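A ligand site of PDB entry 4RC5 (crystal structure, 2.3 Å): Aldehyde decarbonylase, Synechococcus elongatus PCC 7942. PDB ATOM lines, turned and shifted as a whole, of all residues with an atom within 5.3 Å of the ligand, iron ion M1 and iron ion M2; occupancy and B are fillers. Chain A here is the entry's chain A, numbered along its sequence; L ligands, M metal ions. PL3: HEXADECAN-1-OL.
The side-chain carboxylate (OE2) of Glu 105 sits close to the side-chain hydroxyl (OH) of Tyr 29, 3.2 Å away.
The backbone NH (N) of Glu 105 sits at hydrogen-bond distance from the backbone carbonyl oxygen (O) of Gln 100 (3.0 Å).
The side-chain hydroxyl (OH) of Tyr 115 is in hydrogen-bond range of the side-chain hydroxyl (OH) of Tyr 11, 2.9 Å away.
The side-chain carboxylate (OE2) of Glu 22 sits close to the side-chain hydroxyl (OH) of Tyr 112, at 3.5 Å.
Iron ion M2 is bound by OE2 of Glu 105 (2.0 Å), OE2 of Glu 50 (2.1 Å), O1 of the ligand (2.3 Å) and ND1 of His 137 (2.3 Å).
Slightly farther from iron ion M2 lies OE1 of Glu 105 (2.7 Å).
Glu 134 touches iron ion M1.
The nearest printed residue that does not touch iron ion M1 is His 137 (4.5 Å).
Residues that only touch the ligand: Tyr 115, Ala 111, Val 18, Phe 107, Tyr 11, Ile 14, Gln 100, Gly 21, Tyr 112, Ile 104, Ala 108, Ile 17, Ala 25 and Phe 77.
Hydrophobic or aromatic side chains that line the ligand: Ile 14, Ile 17, Val 18, Ala 25, Phe 77, Ile 104, Phe 107, Ala 108, Ala 111, Tyr 112 and Tyr 115.
17 residues have an atom within 4 Å of the ligand: Tyr 11, Ile 14, Ile 17, Val 18, Gly 21, Glu 22, Ala 25, Glu 50, Phe 77, Gln 100, Ile 104, Glu 105, Phe 107, Ala 108, Ala 111, Tyr 112 and Tyr 115.
The nearest printed residue that does not touch the ligand is Val 174 (4.02 Å).
Within 4 Å of iron ion M2: Glu 50, Glu 105 and His 137.
Iron ion M1 is bound by OE1 of Glu 50 (2.0 Å), OE1 of Glu 22 (2.0 Å), ND1 of His 53 (2.4 Å) and OE2 of Glu 22 (2.4 Å).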
ATOM      1  N   TYR A  11      12.883   3.109   7.980  1.00  0.00           N
ATOM      2  CA  TYR A  11      13.290   1.717   7.991  1.00  0.00           C
ATOM      3  C   TYR A  11      12.609   0.956   9.129  1.00  0.00           C
ATOM      4  O   TYR A  11      12.256  -0.231   8.990  1.00  0.00           O
ATOM      5  CB  TYR A  11      14.827   1.550   8.061  1.00  0.00           C
ATOM      6  CG  TYR A  11      15.256   0.288   7.385  1.00  0.00           C
ATOM      7  CD1 TYR A  11      15.455   0.239   5.993  1.00  0.00           C
ATOM      8  CD2 TYR A  11      15.399  -0.895   8.094  1.00  0.00           C
ATOM      9  CE1 TYR A  11      15.827  -0.932   5.368  1.00  0.00           C
ATOM     10  CE2 TYR A  11      15.771  -2.075   7.458  1.00  0.00           C
ATOM     11  CZ  TYR A  11      15.988  -2.069   6.093  1.00  0.00           C
ATOM     12  OH  TYR A  11      16.352  -3.266   5.481  1.00  0.00           O
ATOM     13  N   ILE A  14       9.223   0.071   7.525  1.00  0.00           N
ATOM     14  CA  ILE A  14       9.350  -0.773   6.338  1.00  0.00           C
ATOM     15  C   ILE A  14       9.881  -2.141   6.705  1.00  0.00           C
ATOM     16  O   ILE A  14       9.360  -3.153   6.261  1.00  0.00           O
ATOM     17  CB  ILE A  14      10.292  -0.171   5.267  1.00  0.00           C
ATOM     18  CG1 ILE A  14       9.702   1.079   4.664  1.00  0.00           C
ATOM     19  CG2 ILE A  14      10.598  -1.206   4.156  1.00  0.00           C
ATOM     20  CD1 ILE A  14       8.556   0.861   3.751  1.00  0.00           C
ATOM     21  N   ASN A  15      10.933  -2.174   7.499  1.00  0.00           N
ATOM     22  CA  ASN A  15      11.473  -3.429   8.003  1.00  0.00           C
ATOM     23  C   ASN A  15      10.432  -4.239   8.775  1.00  0.00           C
ATOM     24  O   ASN A  15      10.322  -5.459   8.611  1.00  0.00           O
ATOM     25  CB  ASN A  15      12.644  -3.134   8.905  1.00  0.00           C
ATOM     26  CG  ASN A  15      13.335  -4.390   9.383  1.00  0.00           C
ATOM     27  OD1 ASN A  15      13.571  -4.539  10.588  1.00  0.00           O
ATOM     28  ND2 ASN A  15      13.680  -5.273   8.459  1.00  0.00           N
ATOM     29  N   ILE A  17       7.124  -3.954   8.469  1.00  0.00           N
ATOM     30  CA  ILE A  17       6.080  -4.359   7.533  1.00  0.00           C
ATOM     31  C   ILE A  17       6.506  -5.596   6.761  1.00  0.00           C
ATOM     32  O   ILE A  17       5.713  -6.546   6.605  1.00  0.00           O
ATOM     33  CB  ILE A  17       5.741  -3.236   6.536  1.00  0.00           C
ATOM     34  CG1 ILE A  17       4.748  -2.250   7.174  1.00  0.00           C
ATOM     35  CG2 ILE A  17       5.171  -3.814   5.259  1.00  0.00           C
ATOM     36  CD1 ILE A  17       4.654  -0.923   6.434  1.00  0.00           C
ATOM     37  N   VAL A  18       7.743  -5.597   6.287  1.00  0.00           N
ATOM     38  CA  VAL A  18       8.275  -6.725   5.532  1.00  0.00           C
ATOM     39  C   VAL A  18       8.326  -7.975   6.402  1.00  0.00           C
ATOM     40  O   VAL A  18       7.983  -9.062   5.968  1.00  0.00           O
ATOM     41  CB  VAL A  18       9.677  -6.415   4.976  1.00  0.00           C
ATOM     42  CG1 VAL A  18      10.526  -7.673   4.988  1.00  0.00           C
ATOM     43  CG2 VAL A  18       9.571  -5.827   3.558  1.00  0.00           C
ATOM     44  N   GLY A  21       4.925  -9.465   6.841  1.00  0.00           N
ATOM     45  CA  GLY A  21       4.512 -10.149   5.630  1.00  0.00           C
ATOM     46  C   GLY A  21       5.066 -11.541   5.549  1.00  0.00           C
ATOM     47  O   GLY A  21       4.348 -12.483   5.219  1.00  0.00           O
ATOM     48  N   GLU A  22       6.355 -11.679   5.845  1.00  0.00           N
ATOM     49  CA  GLU A  22       7.020 -12.977   5.814  1.00  0.00           C
ATOM     50  C   GLU A  22       6.448 -13.890   6.889  1.00  0.00           C
ATOM     51  O   GLU A  22       6.173 -15.058   6.640  1.00  0.00           O
ATOM     52  CB  GLU A  22       8.531 -12.811   5.997  1.00  0.00           C
ATOM     53  CG  GLU A  22       9.229 -12.130   4.825  1.00  0.00           C
ATOM     54  CD  GLU A  22       8.970 -12.815   3.514  1.00  0.00           C
ATOM     55  OE1 GLU A  22       8.555 -13.995   3.518  1.00  0.00           O
ATOM     56  OE2 GLU A  22       9.178 -12.180   2.452  1.00  0.00           O
ATOM     57  N   ALA A  25       2.863 -14.715   6.038  1.00  0.00           N
ATOM     58  CA  ALA A  25       2.871 -15.646   4.908  1.00  0.00           C
ATOM     59  C   ALA A  25       3.091 -17.083   5.398  1.00  0.00           C
ATOM     60  O   ALA A  25       2.505 -18.025   4.863  1.00  0.00           O
ATOM     61  CB  ALA A  25       3.923 -15.266   3.892  1.00  0.00           C
ATOM     62  N   TYR A  29       0.480 -20.104   4.244  1.00  0.00           N
ATOM     63  CA  TYR A  29       0.845 -21.356   3.569  1.00  0.00           C
ATOM     64  C   TYR A  29       0.596 -22.627   4.406  1.00  0.00           C
ATOM     65  O   TYR A  29       0.108 -23.611   3.853  1.00  0.00           O
ATOM     66  CB  TYR A  29       2.237 -21.313   2.973  1.00  0.00           C
ATOM     67  CG  TYR A  29       2.293 -20.405   1.775  1.00  0.00           C
ATOM     68  CD1 TYR A  29       1.470 -20.618   0.673  1.00  0.00           C
ATOM     69  CD2 TYR A  29       3.185 -19.335   1.750  1.00  0.00           C
ATOM     70  CE1 TYR A  29       1.533 -19.777  -0.429  1.00  0.00           C
ATOM     71  CE2 TYR A  29       3.255 -18.473   0.649  1.00  0.00           C
ATOM     72  CZ  TYR A  29       2.425 -18.703  -0.429  1.00  0.00           C
ATOM     73  OH  TYR A  29       2.494 -17.873  -1.512  1.00  0.00           O
ATOM     74  N   GLU A  50       9.110 -18.980   3.933  1.00  0.00           N
ATOM     75  CA  GLU A  50       8.724 -17.702   4.549  1.00  0.00           C
ATOM     76  C   GLU A  50       9.401 -17.467   5.930  1.00  0.00           C
ATOM     77  O   GLU A  50       9.811 -16.339   6.253  1.00  0.00           O
ATOM     78  CB  GLU A  50       7.193 -17.565   4.655  1.00  0.00           C
ATOM     79  CG  GLU A  50       6.438 -17.825   3.361  1.00  0.00           C
ATOM     80  CD  GLU A  50       6.626 -16.741   2.301  1.00  0.00           C
ATOM     81  OE1 GLU A  50       7.610 -15.949   2.342  1.00  0.00           O
ATOM     82  OE2 GLU A  50       5.752 -16.665   1.378  1.00  0.00           O
ATOM     83  N   HIS A  53      12.767 -16.148   5.387  1.00  0.00           N
ATOM     84  CA  HIS A  53      12.729 -14.750   4.979  1.00  0.00           C
ATOM     85  C   HIS A  53      12.569 -13.864   6.157  1.00  0.00           C
ATOM     86  O   HIS A  53      13.210 -12.815   6.214  1.00  0.00           O
ATOM     87  CB  HIS A  53      11.559 -14.453   4.039  1.00  0.00           C
ATOM     88  CG  HIS A  53      11.567 -15.290   2.798  1.00  0.00           C
ATOM     89  ND1 HIS A  53      10.513 -15.358   1.999  1.00  0.00           N
ATOM     90  CD2 HIS A  53      12.543 -16.114   2.252  1.00  0.00           C
ATOM     91  CE1 HIS A  53      10.787 -16.184   0.958  1.00  0.00           C
ATOM     92  NE2 HIS A  53      12.033 -16.649   1.126  1.00  0.00           N
ATOM     93  N   PHE A  57      15.055 -10.835   7.264  1.00  0.00           N
ATOM     94  CA  PHE A  57      14.723  -9.418   7.458  1.00  0.00           C
ATOM     95  C   PHE A  57      14.849  -8.899   8.894  1.00  0.00           C
ATOM     96  O   PHE A  57      15.159  -7.733   9.107  1.00  0.00           O
ATOM     97  CB  PHE A  57      13.335  -9.102   6.883  1.00  0.00           C
ATOM     98  CG  PHE A  57      13.330  -9.112   5.378  1.00  0.00           C
ATOM     99  CD1 PHE A  57      14.175  -8.250   4.661  1.00  0.00           C
ATOM    100  CD2 PHE A  57      12.524 -10.009   4.679  1.00  0.00           C
ATOM    101  CE1 PHE A  57      14.184  -8.277   3.284  1.00  0.00           C
ATOM    102  CE2 PHE A  57      12.517 -10.018   3.286  1.00  0.00           C
ATOM    103  CZ  PHE A  57      13.355  -9.154   2.577  1.00  0.00           C
ATOM    104  N   PHE A  76      -0.993  -2.314   9.580  1.00  0.00           N
ATOM    105  CA  PHE A  76      -0.823  -2.276   8.082  1.00  0.00           C
ATOM    106  C   PHE A  76      -1.474  -3.474   7.413  1.00  0.00           C
ATOM    107  O   PHE A  76      -2.206  -3.322   6.416  1.00  0.00           O
ATOM    108  CB  PHE A  76       0.682  -2.251   7.768  1.00  0.00           C
ATOM    109  CG  PHE A  76       1.038  -2.090   6.296  1.00  0.00           C
ATOM    110  CD1 PHE A  76       0.974  -0.832   5.682  1.00  0.00           C
ATOM    111  CD2 PHE A  76       1.517  -3.184   5.558  1.00  0.00           C
ATOM    112  CE1 PHE A  76       1.354  -0.674   4.344  1.00  0.00           C
ATOM    113  CE2 PHE A  76       1.881  -3.021   4.207  1.00  0.00           C
ATOM    114  CZ  PHE A  76       1.811  -1.752   3.612  1.00  0.00           C
ATOM    115  N   PHE A  77      -1.240  -4.650   7.985  1.00  0.00           N
ATOM    116  CA  PHE A  77      -1.675  -5.920   7.419  1.00  0.00           C
ATOM    117  C   PHE A  77      -3.054  -6.413   7.854  1.00  0.00           C
ATOM    118  O   PHE A  77      -3.602  -7.329   7.240  1.00  0.00           O
ATOM    119  CB  PHE A  77      -0.654  -7.019   7.782  1.00  0.00           C
ATOM    120  CG  PHE A  77       0.417  -7.179   6.770  1.00  0.00           C
ATOM    121  CD1 PHE A  77       0.161  -7.848   5.548  1.00  0.00           C
ATOM    122  CD2 PHE A  77       1.679  -6.668   6.994  1.00  0.00           C
ATOM    123  CE1 PHE A  77       1.149  -7.985   4.608  1.00  0.00           C
ATOM    124  CE2 PHE A  77       2.679  -6.809   6.039  1.00  0.00           C
ATOM    125  CZ  PHE A  77       2.411  -7.469   4.856  1.00  0.00           C
ATOM    126  N   GLN A 100      -2.726 -14.566  -0.841  1.00  0.00           N
ATOM    127  CA  GLN A 100      -1.364 -14.832  -0.564  1.00  0.00           C
ATOM    128  C   GLN A 100      -0.470 -15.109  -1.749  1.00  0.00           C
ATOM    129  O   GLN A 100       0.512 -14.469  -1.931  1.00  0.00           O
ATOM    130  CB  GLN A 100      -1.211 -15.916   0.500  1.00  0.00           C
ATOM    131  CG  GLN A 100       0.225 -16.259   0.761  1.00  0.00           C
ATOM    132  CD  GLN A 100       1.025 -15.150   1.397  1.00  0.00           C
ATOM    133  OE1 GLN A 100       0.569 -14.481   2.244  1.00  0.00           O
ATOM    134  NE2 GLN A 100       2.216 -15.007   1.023  1.00  0.00           N
ATOM    135  N   ILE A 104      -0.602 -10.760  -2.852  1.00  0.00           N
ATOM    136  CA  ILE A 104       0.509 -10.532  -1.930  1.00  0.00           C
ATOM    137  C   ILE A 104       1.902 -10.862  -2.405  1.00  0.00           C
ATOM    138  O   ILE A 104       2.751 -10.063  -2.277  1.00  0.00           O
ATOM    139  CB  ILE A 104       0.303 -11.183  -0.544  1.00  0.00           C
ATOM    140  CG1 ILE A 104      -0.722 -10.407   0.268  1.00  0.00           C
ATOM    141  CG2 ILE A 104       1.571 -11.289   0.315  1.00  0.00           C
ATOM    142  CD1 ILE A 104      -0.985 -11.028   1.617  1.00  0.00           C
ATOM    143  N   GLU A 105       2.151 -12.100  -2.803  1.00  0.00           N
ATOM    144  CA  GLU A 105       3.437 -12.449  -3.394  1.00  0.00           C
ATOM    145  C   GLU A 105       3.860 -11.373  -4.389  1.00  0.00           C
ATOM    146  O   GLU A 105       4.919 -10.765  -4.251  1.00  0.00           O
ATOM    147  CB  GLU A 105       3.328 -13.803  -4.090  1.00  0.00           C
ATOM    148  CG  GLU A 105       3.285 -14.984  -3.140  1.00  0.00           C
ATOM    149  CD  GLU A 105       4.536 -15.108  -2.303  1.00  0.00           C
ATOM    150  OE1 GLU A 105       5.635 -14.910  -2.849  1.00  0.00           O
ATOM    151  OE2 GLU A 105       4.422 -15.399  -1.091  1.00  0.00           O
ATOM    152  N   PHE A 107       3.025  -8.387  -4.776  1.00  0.00           N
ATOM    153  CA  PHE A 107       3.347  -7.136  -4.101  1.00  0.00           C
ATOM    154  C   PHE A 107       4.788  -7.146  -3.577  1.00  0.00           C
ATOM    155  O   PHE A 107       5.496  -6.154  -3.686  1.00  0.00           O
ATOM    156  CB  PHE A 107       2.372  -6.891  -2.945  1.00  0.00           C
ATOM    157  CG  PHE A 107       2.507  -5.531  -2.320  1.00  0.00           C
ATOM    158  CD1 PHE A 107       2.699  -4.407  -3.105  1.00  0.00           C
ATOM    159  CD2 PHE A 107       2.454  -5.379  -0.940  1.00  0.00           C
ATOM    160  CE1 PHE A 107       2.822  -3.150  -2.531  1.00  0.00           C
ATOM    161  CE2 PHE A 107       2.582  -4.128  -0.361  1.00  0.00           C
ATOM    162  CZ  PHE A 107       2.769  -3.022  -1.159  1.00  0.00           C
ATOM    163  N   ALA A 108       5.196  -8.270  -3.011  1.00  0.00           N
ATOM    164  CA  ALA A 108       6.542  -8.411  -2.468  1.00  0.00           C
ATOM    165  C   ALA A 108       7.583  -8.447  -3.581  1.00  0.00           C
ATOM    166  O   ALA A 108       8.713  -7.985  -3.408  1.00  0.00           O
ATOM    167  CB  ALA A 108       6.639  -9.655  -1.603  1.00  0.00           C
ATOM    168  N   ALA A 111       8.054  -4.731  -4.969  1.00  0.00           N
ATOM    169  CA  ALA A 111       8.689  -3.864  -3.972  1.00  0.00           C
ATOM    170  C   ALA A 111      10.104  -4.327  -3.663  1.00  0.00           C
ATOM    171  O   ALA A 111      11.048  -3.532  -3.615  1.00  0.00           O
ATOM    172  CB  ALA A 111       7.868  -3.845  -2.701  1.00  0.00           C
ATOM    173  N   TYR A 112      10.259  -5.619  -3.432  1.00  0.00           N
ATOM    174  CA  TYR A 112      11.572  -6.178  -3.219  1.00  0.00           C
ATOM    175  C   TYR A 112      12.533  -5.893  -4.360  1.00  0.00           C
ATOM    176  O   TYR A 112      13.654  -5.480  -4.107  1.00  0.00           O
ATOM    177  CB  TYR A 112      11.489  -7.662  -2.897  1.00  0.00           C
ATOM    178  CG  TYR A 112      10.858  -7.931  -1.560  1.00  0.00           C
ATOM    179  CD1 TYR A 112      10.187  -6.939  -0.857  1.00  0.00           C
ATOM    180  CD2 TYR A 112      10.901  -9.196  -1.025  1.00  0.00           C
ATOM    181  CE1 TYR A 112       9.594  -7.195   0.366  1.00  0.00           C
ATOM    182  CE2 TYR A 112      10.318  -9.468   0.222  1.00  0.00           C
ATOM    183  CZ  TYR A 112       9.671  -8.461   0.902  1.00  0.00           C
ATOM    184  OH  TYR A 112       9.060  -8.739   2.117  1.00  0.00           O
ATOM    185  N   TYR A 115      13.520  -2.389  -4.099  1.00  0.00           N
ATOM    186  CA  TYR A 115      14.395  -2.154  -2.988  1.00  0.00           C
ATOM    187  C   TYR A 115      15.868  -2.567  -3.258  1.00  0.00           C
ATOM    188  O   TYR A 115      16.799  -1.877  -2.827  1.00  0.00           O
ATOM    189  CB  TYR A 115      13.839  -2.807  -1.727  1.00  0.00           C
ATOM    190  CG  TYR A 115      14.754  -2.756  -0.520  1.00  0.00           C
ATOM    191  CD1 TYR A 115      15.131  -1.526   0.061  1.00  0.00           C
ATOM    192  CD2 TYR A 115      15.219  -3.933   0.074  1.00  0.00           C
ATOM    193  CE1 TYR A 115      15.973  -1.500   1.167  1.00  0.00           C
ATOM    194  CE2 TYR A 115      16.032  -3.899   1.182  1.00  0.00           C
ATOM    195  CZ  TYR A 115      16.404  -2.686   1.712  1.00  0.00           C
ATOM    196  OH  TYR A 115      17.234  -2.675   2.813  1.00  0.00           O
ATOM    197  N   THR A 127      17.832  -9.803   0.461  1.00  0.00           N
ATOM    198  CA  THR A 127      16.664  -9.596  -0.383  1.00  0.00           C
ATOM    199  C   THR A 127      16.733 -10.362  -1.732  1.00  0.00           C
ATOM    200  O   THR A 127      15.747 -10.915  -2.170  1.00  0.00           O
ATOM    201  CB  THR A 127      16.392  -8.075  -0.599  1.00  0.00           C
ATOM    202  OG1 THR A 127      16.339  -7.420   0.697  1.00  0.00           O
ATOM    203  CG2 THR A 127      15.077  -7.812  -1.362  1.00  0.00           C
ATOM    204  N   GLU A 134      10.128 -15.979  -3.919  1.00  0.00           N
ATOM    205  CA  GLU A 134       8.830 -15.420  -4.236  1.00  0.00           C
ATOM    206  C   GLU A 134       8.341 -15.802  -5.609  1.00  0.00           C
ATOM    207  O   GLU A 134       7.146 -16.017  -5.782  1.00  0.00           O
ATOM    208  CB  GLU A 134       8.830 -13.875  -4.047  1.00  0.00           C
ATOM    209  CG  GLU A 134       9.312 -13.524  -2.648  1.00  0.00           C
ATOM    210  CD  GLU A 134       9.137 -12.088  -2.263  1.00  0.00           C
ATOM    211  OE1 GLU A 134       9.362 -11.178  -3.104  1.00  0.00           O
ATOM    212  OE2 GLU A 134       8.807 -11.884  -1.054  1.00  0.00           O
ATOM    213  N   HIS A 137       6.588 -19.064  -5.178  1.00  0.00           N
ATOM    214  CA  HIS A 137       5.306 -18.986  -4.500  1.00  0.00           C
ATOM    215  C   HIS A 137       4.219 -18.523  -5.426  1.00  0.00           C
ATOM    216  O   HIS A 137       3.158 -19.116  -5.454  1.00  0.00           O
ATOM    217  CB  HIS A 137       5.396 -17.986  -3.335  1.00  0.00           C
ATOM    218  CG  HIS A 137       6.424 -18.348  -2.310  1.00  0.00           C
ATOM    219  ND1 HIS A 137       6.591 -17.640  -1.189  1.00  0.00           N
ATOM    220  CD2 HIS A 137       7.326 -19.431  -2.244  1.00  0.00           C
ATOM    221  CE1 HIS A 137       7.576 -18.232  -0.453  1.00  0.00           C
ATOM    222  NE2 HIS A 137       8.013 -19.301  -1.101  1.00  0.00           N
ATOM    223  N   VAL A 174       2.569   2.872   2.475  1.00  0.00           N
ATOM    224  CA  VAL A 174       4.033   2.777   2.538  1.00  0.00           C
ATOM    225  C   VAL A 174       4.740   3.841   1.698  1.00  0.00           C
ATOM    226  O   VAL A 174       5.958   4.003   1.824  1.00  0.00           O
ATOM    227  CB  VAL A 174       4.621   1.418   2.080  1.00  0.00           C
ATOM    228  CG1 VAL A 174       4.400   0.348   3.099  1.00  0.00           C
ATOM    229  CG2 VAL A 174       4.149   0.993   0.717  1.00  0.00           C
ATOM    230  N   LEU A 181      13.601   5.517   1.583  1.00  0.00           N
ATOM    231  CA  LEU A 181      14.518   4.403   1.310  1.00  0.00           C
ATOM    232  C   LEU A 181      15.031   4.347  -0.149  1.00  0.00           C
ATOM    233  O   LEU A 181      15.799   3.449  -0.519  1.00  0.00           O
ATOM    234  CB  LEU A 181      13.831   3.078   1.672  1.00  0.00           C
ATOM    235  CG  LEU A 181      14.013   2.506   3.068  1.00  0.00           C
ATOM    236  CD1 LEU A 181      13.476   3.459   4.099  1.00  0.00           C
ATOM    237  CD2 LEU A 181      13.331   1.152   3.212  1.00  0.00           C
ATOM    238  N   MET A 183      12.920   4.360  -2.967  1.00  0.00           N
ATOM    239  CA  MET A 183      11.992   3.581  -3.771  1.00  0.00           C
ATOM    240  C   MET A 183      10.826   4.466  -4.250  1.00  0.00           C
ATOM    241  O   MET A 183      10.025   4.899  -3.435  1.00  0.00           O
ATOM    242  CB  MET A 183      11.439   2.407  -2.956  1.00  0.00           C
ATOM    243  CG  MET A 183      12.462   1.507  -2.316  1.00  0.00           C
ATOM    244  SD  MET A 183      11.725   0.088  -1.449  1.00  0.00           S
ATOM    245  CE  MET A 183      11.164   0.777   0.067  1.00  0.00           C
HETATM  246  C1  PL3 L   1       5.851 -12.777   1.621  1.00  0.00           C
HETATM  247  O1  PL3 L   1       5.556 -13.695   0.842  1.00  0.00           O
HETATM  248  C2  PL3 L   1       4.922 -11.566   1.762  1.00  0.00           C
HETATM  249  C3  PL3 L   1       5.624 -10.265   2.116  1.00  0.00           C
HETATM  250  C4  PL3 L   1       4.899  -9.041   1.581  1.00  0.00           C
HETATM  251  C5  PL3 L   1       5.331  -7.752   2.281  1.00  0.00           C
HETATM  252  C6  PL3 L   1       5.085  -6.568   1.315  1.00  0.00           C
HETATM  253  C7  PL3 L   1       5.665  -5.251   1.880  1.00  0.00           C
HETATM  254  C8  PL3 L   1       5.784  -4.231   0.781  1.00  0.00           C
HETATM  255  C9  PL3 L   1       6.081  -2.866   1.375  1.00  0.00           C
HETATM  256  CA  PL3 L   1       7.427  -2.233   0.949  1.00  0.00           C
HETATM  257  CB  PL3 L   1       8.484  -3.252   0.518  1.00  0.00           C
HETATM  258  CC  PL3 L   1       9.749  -3.226   1.347  1.00  0.00           C
HETATM  259  CD  PL3 L   1      11.008  -3.703   0.623  1.00  0.00           C
HETATM  260  CE  PL3 L   1      12.260  -3.477   1.474  1.00  0.00           C
HETATM  261  CF  PL3 L   1      12.529  -4.581   2.490  1.00  0.00           C
HETATM  262  CG  PL3 L   1      13.493  -4.162   3.630  1.00  0.00           C
HETATM  263 FE    FE M   1       8.447 -14.332   1.546  1.00  0.00          FE
HETATM  264 FE    FE M   2       6.292 -15.556  -0.274  1.00  0.00          FE
